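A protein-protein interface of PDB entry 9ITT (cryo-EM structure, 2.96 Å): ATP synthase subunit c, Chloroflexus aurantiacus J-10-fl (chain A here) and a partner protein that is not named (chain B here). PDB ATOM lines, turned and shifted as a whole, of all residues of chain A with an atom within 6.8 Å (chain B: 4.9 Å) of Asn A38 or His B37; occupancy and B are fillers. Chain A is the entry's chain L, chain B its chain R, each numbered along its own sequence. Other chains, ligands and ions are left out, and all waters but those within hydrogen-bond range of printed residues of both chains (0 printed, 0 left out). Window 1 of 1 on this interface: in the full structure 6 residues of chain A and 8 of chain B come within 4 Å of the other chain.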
ATOM      1  N   ALA A  31      -3.544  24.315  -5.681  1.00  0.00           N
ATOM      2  CA  ALA A  31      -3.559  24.314  -4.224  1.00  0.00           C
ATOM      3  C   ALA A  31      -4.839  24.935  -3.687  1.00  0.00           C
ATOM      4  O   ALA A  31      -5.427  24.428  -2.728  1.00  0.00           O
ATOM      5  CB  ALA A  31      -2.337  25.058  -3.688  1.00  0.00           C
ATOM      6  N   GLN A  33      -7.716  25.085  -5.265  1.00  0.00           N
ATOM      7  CA  GLN A  33      -8.797  24.147  -5.551  1.00  0.00           C
ATOM      8  C   GLN A  33      -8.823  23.018  -4.528  1.00  0.00           C
ATOM      9  O   GLN A  33      -9.895  22.619  -4.060  1.00  0.00           O
ATOM     10  CB  GLN A  33      -8.647  23.592  -6.967  1.00  0.00           C
ATOM     11  CG  GLN A  33      -9.015  24.581  -8.065  1.00  0.00           C
ATOM     12  CD  GLN A  33      -9.763  23.931  -9.210  1.00  0.00           C
ATOM     13  OE1 GLN A  33      -9.435  22.821  -9.630  1.00  0.00           O
ATOM     14  NE2 GLN A  33     -10.773  24.621  -9.726  1.00  0.00           N
ATOM     15  N   ALA A  34      -7.650  22.494  -4.165  1.00  0.00           N
ATOM     16  CA  ALA A  34      -7.593  21.447  -3.149  1.00  0.00           C
ATOM     17  C   ALA A  34      -8.062  21.966  -1.796  1.00  0.00           C
ATOM     18  O   ALA A  34      -8.741  21.253  -1.049  1.00  0.00           O
ATOM     19  CB  ALA A  34      -6.174  20.889  -3.049  1.00  0.00           C
ATOM     20  N   ILE A  35      -7.700  23.207  -1.459  1.00  0.00           N
ATOM     21  CA  ILE A  35      -8.166  23.814  -0.214  1.00  0.00           C
ATOM     22  C   ILE A  35      -9.685  23.912  -0.216  1.00  0.00           C
ATOM     23  O   ILE A  35     -10.350  23.590   0.775  1.00  0.00           O
ATOM     24  CB  ILE A  35      -7.517  25.198  -0.018  1.00  0.00           C
ATOM     25  CG1 ILE A  35      -6.024  25.065   0.305  1.00  0.00           C
ATOM     26  CG2 ILE A  35      -8.239  25.985   1.075  1.00  0.00           C
ATOM     27  CD1 ILE A  35      -5.705  24.599   1.712  1.00  0.00           C
ATOM     28  N   GLY A  36     -10.255  24.371  -1.331  1.00  0.00           N
ATOM     29  CA  GLY A  36     -11.702  24.410  -1.448  1.00  0.00           C
ATOM     30  C   GLY A  36     -12.321  23.036  -1.290  1.00  0.00           C
ATOM     31  O   GLY A  36     -13.372  22.885  -0.664  1.00  0.00           O
ATOM     32  N   ARG A  37     -11.674  22.013  -1.850  1.00  0.00           N
ATOM     33  CA  ARG A  37     -12.141  20.648  -1.644  1.00  0.00           C
ATOM     34  C   ARG A  37     -12.081  20.276  -0.168  1.00  0.00           C
ATOM     35  O   ARG A  37     -13.061  19.780   0.397  1.00  0.00           O
ATOM     36  CB  ARG A  37     -11.306  19.678  -2.485  1.00  0.00           C
ATOM     37  CG  ARG A  37     -11.878  18.266  -2.590  1.00  0.00           C
ATOM     38  CD  ARG A  37     -13.181  18.242  -3.383  1.00  0.00           C
ATOM     39  NE  ARG A  37     -13.575  16.886  -3.763  1.00  0.00           N
ATOM     40  CZ  ARG A  37     -13.721  16.431  -5.004  1.00  0.00           C
ATOM     41  NH1 ARG A  37     -13.502  17.194  -6.066  1.00  0.00           N
ATOM     42  NH2 ARG A  37     -14.098  15.169  -5.189  1.00  0.00           N
ATOM     43  N   ASN A  38     -10.946  20.540   0.484  1.00  0.00           N
ATOM     44  CA  ASN A  38     -10.761  20.197   1.887  1.00  0.00           C
ATOM     45  C   ASN A  38      -9.831  21.220   2.533  1.00  0.00           C
ATOM     46  O   ASN A  38      -8.672  21.330   2.103  1.00  0.00           O
ATOM     47  CB  ASN A  38     -10.178  18.793   2.041  1.00  0.00           C
ATOM     48  CG  ASN A  38     -11.236  17.713   1.943  1.00  0.00           C
ATOM     49  OD1 ASN A  38     -12.145  17.641   2.771  1.00  0.00           O
ATOM     50  ND2 ASN A  38     -11.125  16.866   0.926  1.00  0.00           N
ATOM     51  N   PRO A  39     -10.285  21.990   3.547  1.00  0.00           N
ATOM     52  CA  PRO A  39      -9.363  22.936   4.194  1.00  0.00           C
ATOM     53  C   PRO A  39      -8.439  22.280   5.209  1.00  0.00           C
ATOM     54  O   PRO A  39      -7.321  22.754   5.428  1.00  0.00           O
ATOM     55  CB  PRO A  39     -10.301  23.943   4.877  1.00  0.00           C
ATOM     56  CG  PRO A  39     -11.677  23.618   4.405  1.00  0.00           C
ATOM     57  CD  PRO A  39     -11.658  22.181   4.040  1.00  0.00           C
ATOM     58  N   GLU A  40      -8.889  21.191   5.835  1.00  0.00           N
ATOM     59  CA  GLU A  40      -8.104  20.564   6.894  1.00  0.00           C
ATOM     60  C   GLU A  40      -6.793  19.981   6.382  1.00  0.00           C
ATOM     61  O   GLU A  40      -5.895  19.711   7.185  1.00  0.00           O
ATOM     62  CB  GLU A  40      -8.922  19.466   7.569  1.00  0.00           C
ATOM     63  CG  GLU A  40      -8.436  19.080   8.960  1.00  0.00           C
ATOM     64  CD  GLU A  40      -8.797  20.107  10.019  1.00  0.00           C
ATOM     65  OE1 GLU A  40      -9.721  20.914   9.784  1.00  0.00           O
ATOM     66  OE2 GLU A  40      -8.155  20.106  11.089  1.00  0.00           O
ATOM     67  N   ILE A  41      -6.659  19.790   5.069  1.00  0.00           N
ATOM     68  CA  ILE A  41      -5.429  19.292   4.464  1.00  0.00           C
ATOM     69  C   ILE A  41      -4.529  20.470   4.091  1.00  0.00           C
ATOM     70  O   ILE A  41      -3.583  20.320   3.308  1.00  0.00           O
ATOM     71  CB  ILE A  41      -5.751  18.413   3.239  1.00  0.00           C
ATOM     72  CG1 ILE A  41      -4.602  17.447   2.926  1.00  0.00           C
ATOM     73  CG2 ILE A  41      -6.094  19.272   2.027  1.00  0.00           C
ATOM     74  CD1 ILE A  41      -4.486  16.284   3.894  1.00  0.00           C
ATOM     75  N   GLU A  42      -4.834  21.654   4.633  1.00  0.00           N
ATOM     76  CA  GLU A  42      -4.055  22.846   4.314  1.00  0.00           C
ATOM     77  C   GLU A  42      -2.606  22.688   4.753  1.00  0.00           C
ATOM     78  O   GLU A  42      -1.681  22.980   3.991  1.00  0.00           O
ATOM     79  CB  GLU A  42      -4.694  24.069   4.977  1.00  0.00           C
ATOM     80  CG  GLU A  42      -3.873  25.355   4.922  1.00  0.00           C
ATOM     81  CD  GLU A  42      -4.597  26.519   5.561  1.00  0.00           C
ATOM     82  OE1 GLU A  42      -5.757  26.335   5.988  1.00  0.00           O
ATOM     83  OE2 GLU A  42      -4.006  27.615   5.648  1.00  0.00           O
ATOM     84  N   VAL A  45      -0.852  20.336   2.240  1.00  0.00           N
ATOM     85  CA  VAL A  45      -0.755  20.714   0.831  1.00  0.00           C
ATOM     86  C   VAL A  45       0.053  21.996   0.676  1.00  0.00           C
ATOM     87  O   VAL A  45       0.701  22.204  -0.356  1.00  0.00           O
ATOM     88  CB  VAL A  45      -2.142  20.872   0.181  1.00  0.00           C
ATOM     89  CG1 VAL A  45      -2.905  19.554   0.220  1.00  0.00           C
ATOM     90  CG2 VAL A  45      -2.936  22.013   0.827  1.00  0.00           C
ATOM     91  N   GLY B  32     -11.398  11.419  -0.504  1.00  0.00           N
ATOM     92  CA  GLY B  32     -11.262  11.513   0.935  1.00  0.00           C
ATOM     93  C   GLY B  32     -11.910  12.781   1.443  1.00  0.00           C
ATOM     94  O   GLY B  32     -11.899  13.802   0.748  1.00  0.00           O
ATOM     95  N   ILE B  33     -12.477  12.736   2.646  1.00  0.00           N
ATOM     96  CA  ILE B  33     -13.249  13.848   3.191  1.00  0.00           C
ATOM     97  C   ILE B  33     -12.715  14.165   4.578  1.00  0.00           C
ATOM     98  O   ILE B  33     -12.678  13.289   5.451  1.00  0.00           O
ATOM     99  CB  ILE B  33     -14.753  13.535   3.261  1.00  0.00           C
ATOM    100  CG1 ILE B  33     -15.278  13.014   1.914  1.00  0.00           C
ATOM    101  CG2 ILE B  33     -15.531  14.764   3.717  1.00  0.00           C
ATOM    102  CD1 ILE B  33     -15.306  14.040   0.801  1.00  0.00           C
ATOM    103  N   LEU B  34     -12.312  15.415   4.780  1.00  0.00           N
ATOM    104  CA  LEU B  34     -11.926  15.962   6.066  1.00  0.00           C
ATOM    105  C   LEU B  34     -12.978  16.968   6.532  1.00  0.00           C
ATOM    106  O   LEU B  34     -13.683  17.544   5.698  1.00  0.00           O
ATOM    107  CB  LEU B  34     -10.544  16.620   5.969  1.00  0.00           C
ATOM    108  CG  LEU B  34      -9.406  15.632   5.689  1.00  0.00           C
ATOM    109  CD1 LEU B  34      -8.161  16.347   5.196  1.00  0.00           C
ATOM    110  CD2 LEU B  34      -9.087  14.809   6.932  1.00  0.00           C
ATOM    111  N   PRO B  35     -13.100  17.213   7.849  1.00  0.00           N
ATOM    112  CA  PRO B  35     -14.378  17.725   8.392  1.00  0.00           C
ATOM    113  C   PRO B  35     -14.957  18.957   7.711  1.00  0.00           C
ATOM    114  O   PRO B  35     -16.183  19.033   7.561  1.00  0.00           O
ATOM    115  CB  PRO B  35     -14.040  18.026   9.862  1.00  0.00           C
ATOM    116  CG  PRO B  35     -12.630  17.613  10.083  1.00  0.00           C
ATOM    117  CD  PRO B  35     -12.187  16.800   8.928  1.00  0.00           C
ATOM    118  N   ARG B  36     -14.135  19.919   7.288  1.00  0.00           N
ATOM    119  CA  ARG B  36     -14.644  21.163   6.720  1.00  0.00           C
ATOM    120  C   ARG B  36     -14.725  21.122   5.196  1.00  0.00           C
ATOM    121  O   ARG B  36     -14.551  22.154   4.535  1.00  0.00           O
ATOM    122  CB  ARG B  36     -13.791  22.339   7.197  1.00  0.00           C
ATOM    123  CG  ARG B  36     -14.052  22.691   8.655  1.00  0.00           C
ATOM    124  CD  ARG B  36     -13.367  23.975   9.084  1.00  0.00           C
ATOM    125  NE  ARG B  36     -13.948  25.140   8.419  1.00  0.00           N
ATOM    126  CZ  ARG B  36     -13.277  26.098   7.786  1.00  0.00           C
ATOM    127  NH1 ARG B  36     -11.953  26.111   7.731  1.00  0.00           N
ATOM    128  NH2 ARG B  36     -13.956  27.080   7.201  1.00  0.00           N
ATOM    129  N   HIS B  37     -15.003  19.950   4.628  1.00  0.00           N
ATOM    130  CA  HIS B  37     -15.139  19.807   3.185  1.00  0.00           C
ATOM    131  C   HIS B  37     -16.243  20.713   2.649  1.00  0.00           C
ATOM    132  O   HIS B  37     -17.259  20.952   3.307  1.00  0.00           O
ATOM    133  CB  HIS B  37     -15.452  18.350   2.838  1.00  0.00           C
ATOM    134  CG  HIS B  37     -15.313  18.023   1.384  1.00  0.00           C
ATOM    135  ND1 HIS B  37     -16.165  18.521   0.423  1.00  0.00           N
ATOM    136  CD2 HIS B  37     -14.436  17.224   0.731  1.00  0.00           C
ATOM    137  CE1 HIS B  37     -15.807  18.060  -0.762  1.00  0.00           C
ATOM    138  NE2 HIS B  37     -14.760  17.270  -0.603  1.00  0.00           N
ATOM    139  N   ALA B  38     -16.031  21.221   1.438  1.00  0.00           N
ATOM    140  CA  ALA B  38     -17.048  22.025   0.785  1.00  0.00           C
ATOM    141  C   ALA B  38     -18.243  21.149   0.416  1.00  0.00           C
ATOM    142  O   ALA B  38     -18.125  19.920   0.372  1.00  0.00           O
ATOM    143  CB  ALA B  38     -16.481  22.688  -0.466  1.00  0.00           C
ATOM    144  N   PRO B  39     -19.412  21.746   0.164  1.00  0.00           N
ATOM    145  CA  PRO B  39     -20.591  20.933  -0.161  1.00  0.00           C
ATOM    146  C   PRO B  39     -20.366  20.084  -1.404  1.00  0.00           C
ATOM    147  O   PRO B  39     -19.746  20.521  -2.376  1.00  0.00           O
ATOM    148  CB  PRO B  39     -21.691  21.977  -0.384  1.00  0.00           C
ATOM    149  CG  PRO B  39     -21.226  23.187   0.329  1.00  0.00           C
ATOM    150  CD  PRO B  39     -19.738  23.182   0.201  1.00  0.00           C
ATOM    151  N   LEU B  40     -20.885  18.857  -1.366  1.00  0.00           N
ATOM    152  CA  LEU B  40     -20.625  17.891  -2.432  1.00  0.00           C
ATOM    153  C   LEU B  40     -21.671  16.791  -2.382  1.00  0.00           C
ATOM    154  O   LEU B  40     -22.069  16.364  -1.293  1.00  0.00           O
ATOM    155  CB  LEU B  40     -19.215  17.309  -2.286  1.00  0.00           C
ATOM    156  CG  LEU B  40     -18.788  16.183  -3.237  1.00  0.00           C
ATOM    157  CD1 LEU B  40     -17.295  16.267  -3.510  1.00  0.00           C
ATOM    158  CD2 LEU B  40     -19.132  14.797  -2.685  1.00  0.00           C
ATOM    159  N   VAL B  69     -22.359  15.940   1.521  1.00  0.00           N
ATOM    160  CA  VAL B  69     -21.310  16.555   2.324  1.00  0.00           C
ATOM    161  C   VAL B  69     -21.675  18.010   2.564  1.00  0.00           C
ATOM    162  O   VAL B  69     -22.177  18.693   1.665  1.00  0.00           O
ATOM    163  CB  VAL B  69     -19.933  16.440   1.641  1.00  0.00           C
ATOM    164  CG1 VAL B  69     -18.826  16.839   2.605  1.00  0.00           C
ATOM    165  CG2 VAL B  69     -19.714  15.026   1.121  1.00  0.00           C
ATOM    166  N   LEU B  70     -21.449  18.473   3.785  1.00  0.00           N
ATOM    167  CA  LEU B  70     -21.616  19.862   4.173  1.00  0.00           C
ATOM    168  C   LEU B  70     -20.500  20.238   5.134  1.00  0.00           C
ATOM    169  O   LEU B  70     -19.881  19.362   5.747  1.00  0.00           O
ATOM    170  CB  LEU B  70     -22.983  20.101   4.835  1.00  0.00           C
ATOM    171  CG  LEU B  70     -24.203  20.006   3.917  1.00  0.00           C
ATOM    172  CD1 LEU B  70     -25.485  20.126   4.722  1.00  0.00           C
ATOM    173  CD2 LEU B  70     -24.161  21.065   2.821  1.00  0.00           C
ATOM    174  N   PRO B  71     -20.203  21.534   5.277  1.00  0.00           N
ATOM    175  CA  PRO B  71     -19.153  21.927   6.231  1.00  0.00           C
ATOM    176  C   PRO B  71     -19.438  21.494   7.657  1.00  0.00           C
ATOM    177  O   PRO B  71     -18.500  21.162   8.392  1.00  0.00           O
ATOM    178  CB  PRO B  71     -19.115  23.459   6.101  1.00  0.00           C
ATOM    179  CG  PRO B  71     -20.420  23.828   5.474  1.00  0.00           C
ATOM    180  CD  PRO B  71     -20.732  22.702   4.552  1.00  0.00           C
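The backbone carbonyl oxygen (O) of Gly B32 is in hydrogen-bond range of the side-chain amide nitrogen (ND2) of Asn A38 (3.2 Å). The side-chain amide oxygen of Asn A38 sits at hydrogen-bond distance from the backbone NH of Leu B34, at 3.0 Å. A ring nitrogen (NE2) of His B37 lies close to the backbone carbonyl oxygen of Arg A37, 3.2 Å away. N of Ala B38 sits at hydrogen-bond distance from O of Arg A37, 3.5 Å away.
The backbone NH (N) of Val B69 lies within hydrogen-bond range of the backbone carbonyl oxygen (O) of Leu B40, at 2.9 Å.
Among the printed residues, merely in contact across the chains: Gly A36 with Ala B38, Arg A37 with Leu B40, Asn A38 with Ile B33, Asn A38 with His B37, Pro A39 with Arg B36, Glu A40 with Leu B34 and Ile A41 with Leu B34.
Of the printed residues of chain B, Arg A37 touches His B37 (2.9 Å), Ala B38 (3.5 Å) and Leu B40 (3.8 Å). Of the printed residues of chain B, Ile A41 touches Leu B34. Printed residues of chain A within 4 Å of Arg B36: Pro A39. His B37 touches two residues of chain A. The nearest printed residue of chain B that does not touch Asn A38 is Arg B36 (5.0 Å).
Of the 12 printed residues of chain A, 6 touch a printed residue of chain B. Among the printed residues, no Asp or Glu carboxylate lies within 4 Å of a Lys or Arg side-chain nitrogen of the other chain.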
